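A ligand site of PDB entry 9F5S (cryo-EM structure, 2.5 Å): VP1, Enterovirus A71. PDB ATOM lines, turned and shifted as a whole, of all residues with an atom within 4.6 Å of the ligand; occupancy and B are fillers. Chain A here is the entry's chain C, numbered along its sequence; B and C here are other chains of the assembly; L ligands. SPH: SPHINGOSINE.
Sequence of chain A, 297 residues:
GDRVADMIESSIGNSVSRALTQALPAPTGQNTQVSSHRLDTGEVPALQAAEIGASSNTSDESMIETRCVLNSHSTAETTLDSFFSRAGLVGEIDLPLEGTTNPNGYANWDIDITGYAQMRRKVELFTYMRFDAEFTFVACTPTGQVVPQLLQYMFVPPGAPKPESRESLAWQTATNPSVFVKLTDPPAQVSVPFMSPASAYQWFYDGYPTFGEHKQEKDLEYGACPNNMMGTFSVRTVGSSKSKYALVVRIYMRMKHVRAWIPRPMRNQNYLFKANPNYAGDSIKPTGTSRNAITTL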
ATOM      1  N   ILE A 111     -22.039   6.431 -28.622  1.00  0.00           N
ATOM      2  CA  ILE A 111     -23.473   6.369 -28.389  1.00  0.00           C
ATOM      3  C   ILE A 111     -24.073   7.746 -28.630  1.00  0.00           C
ATOM      4  O   ILE A 111     -23.777   8.712 -27.922  1.00  0.00           O
ATOM      5  CB  ILE A 111     -23.783   5.874 -26.967  1.00  0.00           C
ATOM      6  CG1 ILE A 111     -23.316   4.420 -26.811  1.00  0.00           C
ATOM      7  CG2 ILE A 111     -25.270   5.978 -26.690  1.00  0.00           C
ATOM      8  CD1 ILE A 111     -22.676   4.131 -25.485  1.00  0.00           C
ATOM      9  N   ASP A 112     -24.925   7.843 -29.649  1.00  0.00           N
ATOM     10  CA  ASP A 112     -25.559   9.094 -30.032  1.00  0.00           C
ATOM     11  C   ASP A 112     -26.813   8.765 -30.818  1.00  0.00           C
ATOM     12  O   ASP A 112     -26.731   8.098 -31.854  1.00  0.00           O
ATOM     13  CB  ASP A 112     -24.605   9.955 -30.866  1.00  0.00           C
ATOM     14  CG  ASP A 112     -25.287  11.144 -31.488  1.00  0.00           C
ATOM     15  OD1 ASP A 112     -25.543  12.137 -30.768  1.00  0.00           O
ATOM     16  OD2 ASP A 112     -25.592  11.100 -32.699  1.00  0.00           O
ATOM     17  N   ILE A 113     -27.966   9.216 -30.328  1.00  0.00           N
ATOM     18  CA  ILE A 113     -29.237   8.837 -30.920  1.00  0.00           C
ATOM     19  C   ILE A 113     -29.667   9.864 -31.960  1.00  0.00           C
ATOM     20  O   ILE A 113     -30.696   9.715 -32.619  1.00  0.00           O
ATOM     21  CB  ILE A 113     -30.324   8.667 -29.846  1.00  0.00           C
ATOM     22  CG1 ILE A 113     -30.903  10.026 -29.439  1.00  0.00           C
ATOM     23  CG2 ILE A 113     -29.750   7.943 -28.628  1.00  0.00           C
ATOM     24  CD1 ILE A 113     -31.833   9.976 -28.259  1.00  0.00           C
ATOM     25  N   THR A 114     -28.859  10.919 -32.124  1.00  0.00           N
ATOM     26  CA  THR A 114     -29.182  12.000 -33.038  1.00  0.00           C
ATOM     27  C   THR A 114     -28.743  11.717 -34.467  1.00  0.00           C
ATOM     28  O   THR A 114     -28.625  12.646 -35.271  1.00  0.00           O
ATOM     29  CB  THR A 114     -28.551  13.320 -32.552  1.00  0.00           C
ATOM     30  OG1 THR A 114     -27.128  13.242 -32.671  1.00  0.00           O
ATOM     31  CG2 THR A 114     -28.935  13.580 -31.105  1.00  0.00           C
ATOM     32  N   PHE A 131     -34.268   9.627 -18.699  1.00  0.00           N
ATOM     33  CA  PHE A 131     -34.983   8.377 -18.939  1.00  0.00           C
ATOM     34  C   PHE A 131     -34.033   7.210 -18.745  1.00  0.00           C
ATOM     35  O   PHE A 131     -32.808   7.367 -18.723  1.00  0.00           O
ATOM     36  CB  PHE A 131     -35.594   8.333 -20.342  1.00  0.00           C
ATOM     37  CG  PHE A 131     -34.627   8.716 -21.442  1.00  0.00           C
ATOM     38  CD1 PHE A 131     -33.676   7.810 -21.900  1.00  0.00           C
ATOM     39  CD2 PHE A 131     -34.682   9.970 -22.019  1.00  0.00           C
ATOM     40  CE1 PHE A 131     -32.797   8.165 -22.903  1.00  0.00           C
ATOM     41  CE2 PHE A 131     -33.812  10.323 -23.026  1.00  0.00           C
ATOM     42  CZ  PHE A 131     -32.867   9.417 -23.471  1.00  0.00           C
ATOM     43  N   PHE A 135     -32.396  -1.078 -24.771  1.00  0.00           N
ATOM     44  CA  PHE A 135     -31.592  -1.101 -25.985  1.00  0.00           C
ATOM     45  C   PHE A 135     -31.711  -2.474 -26.637  1.00  0.00           C
ATOM     46  O   PHE A 135     -31.368  -3.483 -26.026  1.00  0.00           O
ATOM     47  CB  PHE A 135     -30.123  -0.784 -25.662  1.00  0.00           C
ATOM     48  CG  PHE A 135     -29.756   0.647 -25.934  1.00  0.00           C
ATOM     49  CD1 PHE A 135     -30.281   1.671 -25.174  1.00  0.00           C
ATOM     50  CD2 PHE A 135     -28.871   0.959 -26.952  1.00  0.00           C
ATOM     51  CE1 PHE A 135     -29.939   2.975 -25.425  1.00  0.00           C
ATOM     52  CE2 PHE A 135     -28.527   2.270 -27.209  1.00  0.00           C
ATOM     53  CZ  PHE A 135     -29.056   3.280 -26.435  1.00  0.00           C
ATOM     54  N   PHE A 137     -30.654  -4.679 -30.089  1.00  0.00           N
ATOM     55  CA  PHE A 137     -29.703  -4.721 -31.199  1.00  0.00           C
ATOM     56  C   PHE A 137     -30.109  -5.849 -32.133  1.00  0.00           C
ATOM     57  O   PHE A 137     -29.988  -7.032 -31.790  1.00  0.00           O
ATOM     58  CB  PHE A 137     -28.283  -4.924 -30.684  1.00  0.00           C
ATOM     59  CG  PHE A 137     -27.995  -4.191 -29.413  1.00  0.00           C
ATOM     60  CD1 PHE A 137     -27.708  -2.839 -29.421  1.00  0.00           C
ATOM     61  CD2 PHE A 137     -28.019  -4.862 -28.196  1.00  0.00           C
ATOM     62  CE1 PHE A 137     -27.449  -2.162 -28.246  1.00  0.00           C
ATOM     63  CE2 PHE A 137     -27.758  -4.199 -27.021  1.00  0.00           C
ATOM     64  CZ  PHE A 137     -27.473  -2.849 -27.045  1.00  0.00           C
ATOM     65  N   PHE A 155     -20.755  -2.458 -23.861  1.00  0.00           N
ATOM     66  CA  PHE A 155     -20.844  -1.049 -23.516  1.00  0.00           C
ATOM     67  C   PHE A 155     -19.508  -0.579 -22.960  1.00  0.00           C
ATOM     68  O   PHE A 155     -19.024  -1.118 -21.952  1.00  0.00           O
ATOM     69  CB  PHE A 155     -21.964  -0.831 -22.499  1.00  0.00           C
ATOM     70  CG  PHE A 155     -22.015   0.551 -21.923  1.00  0.00           C
ATOM     71  CD1 PHE A 155     -21.971   1.667 -22.740  1.00  0.00           C
ATOM     72  CD2 PHE A 155     -22.110   0.737 -20.556  1.00  0.00           C
ATOM     73  CE1 PHE A 155     -22.018   2.938 -22.206  1.00  0.00           C
ATOM     74  CE2 PHE A 155     -22.164   2.009 -20.010  1.00  0.00           C
ATOM     75  CZ  PHE A 155     -22.119   3.108 -20.843  1.00  0.00           C
ATOM     76  N   PRO A 177     -19.998  -3.768 -19.178  1.00  0.00           N
ATOM     77  CA  PRO A 177     -21.179  -4.567 -19.513  1.00  0.00           C
ATOM     78  C   PRO A 177     -21.098  -5.037 -20.961  1.00  0.00           C
ATOM     79  O   PRO A 177     -20.991  -4.234 -21.886  1.00  0.00           O
ATOM     80  CB  PRO A 177     -22.345  -3.594 -19.301  1.00  0.00           C
ATOM     81  CG  PRO A 177     -21.774  -2.462 -18.514  1.00  0.00           C
ATOM     82  CD  PRO A 177     -20.347  -2.363 -18.931  1.00  0.00           C
ATOM     83  N   VAL A 179     -22.580  -8.077 -23.954  1.00  0.00           N
ATOM     84  CA  VAL A 179     -23.602  -9.027 -24.349  1.00  0.00           C
ATOM     85  C   VAL A 179     -23.012  -9.969 -25.391  1.00  0.00           C
ATOM     86  O   VAL A 179     -22.500  -9.513 -26.421  1.00  0.00           O
ATOM     87  CB  VAL A 179     -24.850  -8.318 -24.908  1.00  0.00           C
ATOM     88  CG1 VAL A 179     -25.945  -9.335 -25.217  1.00  0.00           C
ATOM     89  CG2 VAL A 179     -25.362  -7.276 -23.935  1.00  0.00           C
ATOM     90  N   VAL A 190     -31.344  -5.126 -23.656  1.00  0.00           N
ATOM     91  CA  VAL A 190     -30.766  -4.764 -22.367  1.00  0.00           C
ATOM     92  C   VAL A 190     -31.412  -3.473 -21.885  1.00  0.00           C
ATOM     93  O   VAL A 190     -31.718  -2.583 -22.672  1.00  0.00           O
ATOM     94  CB  VAL A 190     -29.230  -4.584 -22.451  1.00  0.00           C
ATOM     95  CG1 VAL A 190     -28.534  -5.943 -22.477  1.00  0.00           C
ATOM     96  CG2 VAL A 190     -28.850  -3.748 -23.658  1.00  0.00           C
ATOM     97  N   VAL A 192     -30.819  -0.061 -20.132  1.00  0.00           N
ATOM     98  CA  VAL A 192     -29.750   0.896 -19.879  1.00  0.00           C
ATOM     99  C   VAL A 192     -30.302   1.970 -18.955  1.00  0.00           C
ATOM    100  O   VAL A 192     -31.320   2.592 -19.269  1.00  0.00           O
ATOM    101  CB  VAL A 192     -29.223   1.532 -21.187  1.00  0.00           C
ATOM    102  CG1 VAL A 192     -28.206   2.606 -20.867  1.00  0.00           C
ATOM    103  CG2 VAL A 192     -28.630   0.463 -22.081  1.00  0.00           C
ATOM    104  N   MET A 195     -27.727   7.507 -17.602  1.00  0.00           N
ATOM    105  CA  MET A 195     -26.273   7.584 -17.564  1.00  0.00           C
ATOM    106  C   MET A 195     -25.720   8.923 -17.093  1.00  0.00           C
ATOM    107  O   MET A 195     -24.642   8.942 -16.486  1.00  0.00           O
ATOM    108  CB  MET A 195     -25.698   7.296 -18.965  1.00  0.00           C
ATOM    109  CG  MET A 195     -26.031   5.940 -19.636  1.00  0.00           C
ATOM    110  SD  MET A 195     -25.238   4.435 -19.011  1.00  0.00           S
ATOM    111  CE  MET A 195     -25.961   4.168 -17.406  1.00  0.00           C
ATOM    112  N   TYR A 201     -30.596  14.161 -19.654  1.00  0.00           N
ATOM    113  CA  TYR A 201     -29.862  14.295 -20.896  1.00  0.00           C
ATOM    114  C   TYR A 201     -30.203  15.620 -21.556  1.00  0.00           C
ATOM    115  O   TYR A 201     -31.256  16.205 -21.328  1.00  0.00           O
ATOM    116  CB  TYR A 201     -30.170  13.129 -21.847  1.00  0.00           C
ATOM    117  CG  TYR A 201     -29.791  11.776 -21.295  1.00  0.00           C
ATOM    118  CD1 TYR A 201     -28.481  11.495 -20.933  1.00  0.00           C
ATOM    119  CD2 TYR A 201     -30.746  10.775 -21.139  1.00  0.00           C
ATOM    120  CE1 TYR A 201     -28.131  10.254 -20.446  1.00  0.00           C
ATOM    121  CE2 TYR A 201     -30.403   9.534 -20.640  1.00  0.00           C
ATOM    122  CZ  TYR A 201     -29.092   9.282 -20.292  1.00  0.00           C
ATOM    123  OH  TYR A 201     -28.762   8.045 -19.791  1.00  0.00           O
ATOM    124  N   GLN A 202     -29.280  16.097 -22.390  1.00  0.00           N
ATOM    125  CA  GLN A 202     -29.320  17.462 -22.891  1.00  0.00           C
ATOM    126  C   GLN A 202     -29.054  17.427 -24.396  1.00  0.00           C
ATOM    127  O   GLN A 202     -27.897  17.350 -24.828  1.00  0.00           O
ATOM    128  CB  GLN A 202     -28.319  18.322 -22.138  1.00  0.00           C
ATOM    129  CG  GLN A 202     -28.015  19.683 -22.706  1.00  0.00           C
ATOM    130  CD  GLN A 202     -27.672  20.691 -21.633  1.00  0.00           C
ATOM    131  OE1 GLN A 202     -28.367  21.691 -21.456  1.00  0.00           O
ATOM    132  NE2 GLN A 202     -26.602  20.420 -20.892  1.00  0.00           N
ATOM    133  N   TRP A 203     -30.114  17.457 -25.197  1.00  0.00           N
ATOM    134  CA  TRP A 203     -29.960  17.474 -26.644  1.00  0.00           C
ATOM    135  C   TRP A 203     -29.510  18.828 -27.156  1.00  0.00           C
ATOM    136  O   TRP A 203     -29.063  18.927 -28.312  1.00  0.00           O
ATOM    137  CB  TRP A 203     -31.275  17.109 -27.336  1.00  0.00           C
ATOM    138  CG  TRP A 203     -32.100  16.125 -26.584  1.00  0.00           C
ATOM    139  CD1 TRP A 203     -33.306  16.361 -25.996  1.00  0.00           C
ATOM    140  CD2 TRP A 203     -31.767  14.766 -26.301  1.00  0.00           C
ATOM    141  NE1 TRP A 203     -33.757  15.217 -25.382  1.00  0.00           N
ATOM    142  CE2 TRP A 203     -32.826  14.225 -25.553  1.00  0.00           C
ATOM    143  CE3 TRP A 203     -30.682  13.943 -26.610  1.00  0.00           C
ATOM    144  CZ2 TRP A 203     -32.845  12.908 -25.118  1.00  0.00           C
ATOM    145  CZ3 TRP A 203     -30.690  12.636 -26.177  1.00  0.00           C
ATOM    146  CH2 TRP A 203     -31.767  12.134 -25.437  1.00  0.00           C
ATOM    147  N   ASN A 228     -23.907  13.995 -22.147  1.00  0.00           N
ATOM    148  CA  ASN A 228     -24.660  13.176 -23.091  1.00  0.00           C
ATOM    149  C   ASN A 228     -23.830  12.126 -23.805  1.00  0.00           C
ATOM    150  O   ASN A 228     -24.344  11.028 -24.041  1.00  0.00           O
ATOM    151  CB  ASN A 228     -25.342  14.076 -24.136  1.00  0.00           C
ATOM    152  CG  ASN A 228     -26.224  15.131 -23.504  1.00  0.00           C
ATOM    153  OD1 ASN A 228     -27.094  14.823 -22.700  1.00  0.00           O
ATOM    154  ND2 ASN A 228     -25.980  16.384 -23.876  1.00  0.00           N
ATOM    155  N   MET A 229     -22.586  12.422 -24.163  1.00  0.00           N
ATOM    156  CA  MET A 229     -21.710  11.404 -24.757  1.00  0.00           C
ATOM    157  C   MET A 229     -21.267  10.479 -23.635  1.00  0.00           C
ATOM    158  O   MET A 229     -20.280  10.738 -22.945  1.00  0.00           O
ATOM    159  CB  MET A 229     -20.540  12.034 -25.517  1.00  0.00           C
ATOM    160  CG  MET A 229     -19.762  13.140 -24.809  1.00  0.00           C
ATOM    161  SD  MET A 229     -19.502  14.575 -25.870  1.00  0.00           S
ATOM    162  CE  MET A 229     -21.187  15.089 -26.196  1.00  0.00           C
ATOM    163  N   PHE A 233     -20.477   2.080 -27.820  1.00  0.00           N
ATOM    164  CA  PHE A 233     -21.047   0.750 -27.991  1.00  0.00           C
ATOM    165  C   PHE A 233     -20.150  -0.019 -28.952  1.00  0.00           C
ATOM    166  O   PHE A 233     -20.114   0.279 -30.146  1.00  0.00           O
ATOM    167  CB  PHE A 233     -22.475   0.820 -28.515  1.00  0.00           C
ATOM    168  CG  PHE A 233     -23.069  -0.516 -28.817  1.00  0.00           C
ATOM    169  CD1 PHE A 233     -23.487  -1.358 -27.803  1.00  0.00           C
ATOM    170  CD2 PHE A 233     -23.204  -0.937 -30.133  1.00  0.00           C
ATOM    171  CE1 PHE A 233     -24.030  -2.590 -28.099  1.00  0.00           C
ATOM    172  CE2 PHE A 233     -23.747  -2.168 -30.429  1.00  0.00           C
ATOM    173  CZ  PHE A 233     -24.160  -2.994 -29.412  1.00  0.00           C
ATOM    174  N   ALA A 275     -25.890  15.714 -33.315  1.00  0.00           N
ATOM    175  CA  ALA A 275     -25.675  16.638 -32.199  1.00  0.00           C
ATOM    176  C   ALA A 275     -25.362  18.050 -32.696  1.00  0.00           C
ATOM    177  O   ALA A 275     -24.452  18.727 -32.217  1.00  0.00           O
ATOM    178  CB  ALA A 275     -24.575  16.126 -31.263  1.00  0.00           C
ATOM    179  N   ILE B  24     -27.896  -3.811 -17.642  1.00  0.00           N
ATOM    180  CA  ILE B  24     -26.467  -3.896 -17.884  1.00  0.00           C
ATOM    181  C   ILE B  24     -25.647  -3.551 -16.657  1.00  0.00           C
ATOM    182  O   ILE B  24     -24.457  -3.892 -16.594  1.00  0.00           O
ATOM    183  CB  ILE B  24     -26.047  -2.977 -19.052  1.00  0.00           C
ATOM    184  CG1 ILE B  24     -26.613  -1.577 -18.849  1.00  0.00           C
ATOM    185  CG2 ILE B  24     -26.457  -3.566 -20.377  1.00  0.00           C
ATOM    186  CD1 ILE B  24     -25.848  -0.490 -19.578  1.00  0.00           C
ATOM    187  N   LEU C  14     -25.292 -10.669 -21.203  1.00  0.00           N
ATOM    188  CA  LEU C  14     -24.878  -9.409 -20.598  1.00  0.00           C
ATOM    189  C   LEU C  14     -23.928  -9.701 -19.452  1.00  0.00           C
ATOM    190  O   LEU C  14     -24.292 -10.405 -18.500  1.00  0.00           O
ATOM    191  CB  LEU C  14     -26.098  -8.618 -20.121  1.00  0.00           C
ATOM    192  CG  LEU C  14     -25.786  -7.294 -19.415  1.00  0.00           C
ATOM    193  CD1 LEU C  14     -25.087  -6.329 -20.363  1.00  0.00           C
ATOM    194  CD2 LEU C  14     -27.055  -6.669 -18.873  1.00  0.00           C
HETATM  195  C1  SPH L   1     -26.868  14.744 -27.370  1.00  0.00           C
HETATM  196  O1  SPH L   1     -26.984  15.663 -28.433  1.00  0.00           O
HETATM  197  C2  SPH L   1     -26.405  13.394 -27.914  1.00  0.00           C
HETATM  198  N2  SPH L   1     -25.162  12.986 -27.290  1.00  0.00           N
HETATM  199  C3  SPH L   1     -27.500  12.331 -27.814  1.00  0.00           C
HETATM  200  O3  SPH L   1     -27.491  11.497 -28.941  1.00  0.00           O
HETATM  201  C4  SPH L   1     -27.445  11.505 -26.564  1.00  0.00           C
HETATM  202  C5  SPH L   1     -26.613  10.291 -26.477  1.00  0.00           C
HETATM  203  C6  SPH L   1     -27.094   9.062 -25.739  1.00  0.00           C
HETATM  204  C7  SPH L   1     -28.236   9.415 -24.791  1.00  0.00           C
HETATM  205  C8  SPH L   1     -28.295   8.466 -23.595  1.00  0.00           C
HETATM  206  C9  SPH L   1     -28.368   6.996 -23.999  1.00  0.00           C
HETATM  207  C10 SPH L   1     -27.177   6.225 -23.432  1.00  0.00           C
HETATM  208  C11 SPH L   1     -27.318   4.733 -23.712  1.00  0.00           C
HETATM  209  C12 SPH L   1     -25.967   4.021 -23.648  1.00  0.00           C
HETATM  210  C13 SPH L   1     -25.964   2.781 -24.542  1.00  0.00           C
HETATM  211  C14 SPH L   1     -25.522   1.537 -23.758  1.00  0.00           C
HETATM  212  C15 SPH L   1     -25.683   0.280 -24.591  1.00  0.00           C
HETATM  213  C16 SPH L   1     -25.439  -0.968 -23.755  1.00  0.00           C
HETATM  214  C17 SPH L   1     -24.928  -2.117 -24.607  1.00  0.00           C
HETATM  215  C18 SPH L   1     -24.504  -3.303 -23.750  1.00  0.00           C
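The side-chain carboxylate (OD2) of Asp 112 lies within hydrogen-bond range of the side-chain hydroxyl (OG1) of Thr 114 (2.6 Å).
The side-chain hydroxyl of Thr 114 is in hydrogen-bond range of the backbone NH of Ala 275 (2.8 Å).
The side-chain amide oxygen (OD1) of Asn 228 lies within hydrogen-bond range of the backbone NH (N) of Gln 202, 2.5 Å away.
The backbone NH (N) of Met 195 is in hydrogen-bond range of the side-chain hydroxyl (OH) of Tyr 201.
The backbone carbonyl oxygen of Val 190 is in hydrogen-bond range of the backbone NH of Phe 135, at 2.7 Å.
N of Phe 155 sits at hydrogen-bond distance from O of Pro 177.
O3 of the ligand lies within hydrogen-bond range of N of Ile 113 (2.7 Å).
The side-chain carboxylate of Asp 112 lies within salt-bridge range of a nitrogen (N2) of the ligand (3.6 Å).
Residues that only touch the ligand: Thr 114 (3.3 Å), Asn 228 (3.3 Å), Trp 203 (3.5 Å), Tyr 201 (3.5 Å), Phe 135 (3.5 Å), Ile 111 (3.6 Å), Phe 233 (3.6 Å), Phe 137 (3.6 Å), Val 192 (3.7 Å), Phe 155 (3.7 Å), Ala 275 (3.7 Å), Gln 202 (3.8 Å), Ile 24 of chain B (3.9 Å) and Met 195 (3.98 Å).
Hydrophobic or aromatic side chains within 4 Å of the ligand: Ile 111, Ile 113, Phe 135, Phe 137, Phe 155, Val 192, Met 195, Tyr 201, Trp 203, Phe 233, Ala 275 and Ile 24 of chain B.
The nearest printed residue that does not touch the ligand is Val 179 (4.1 Å).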
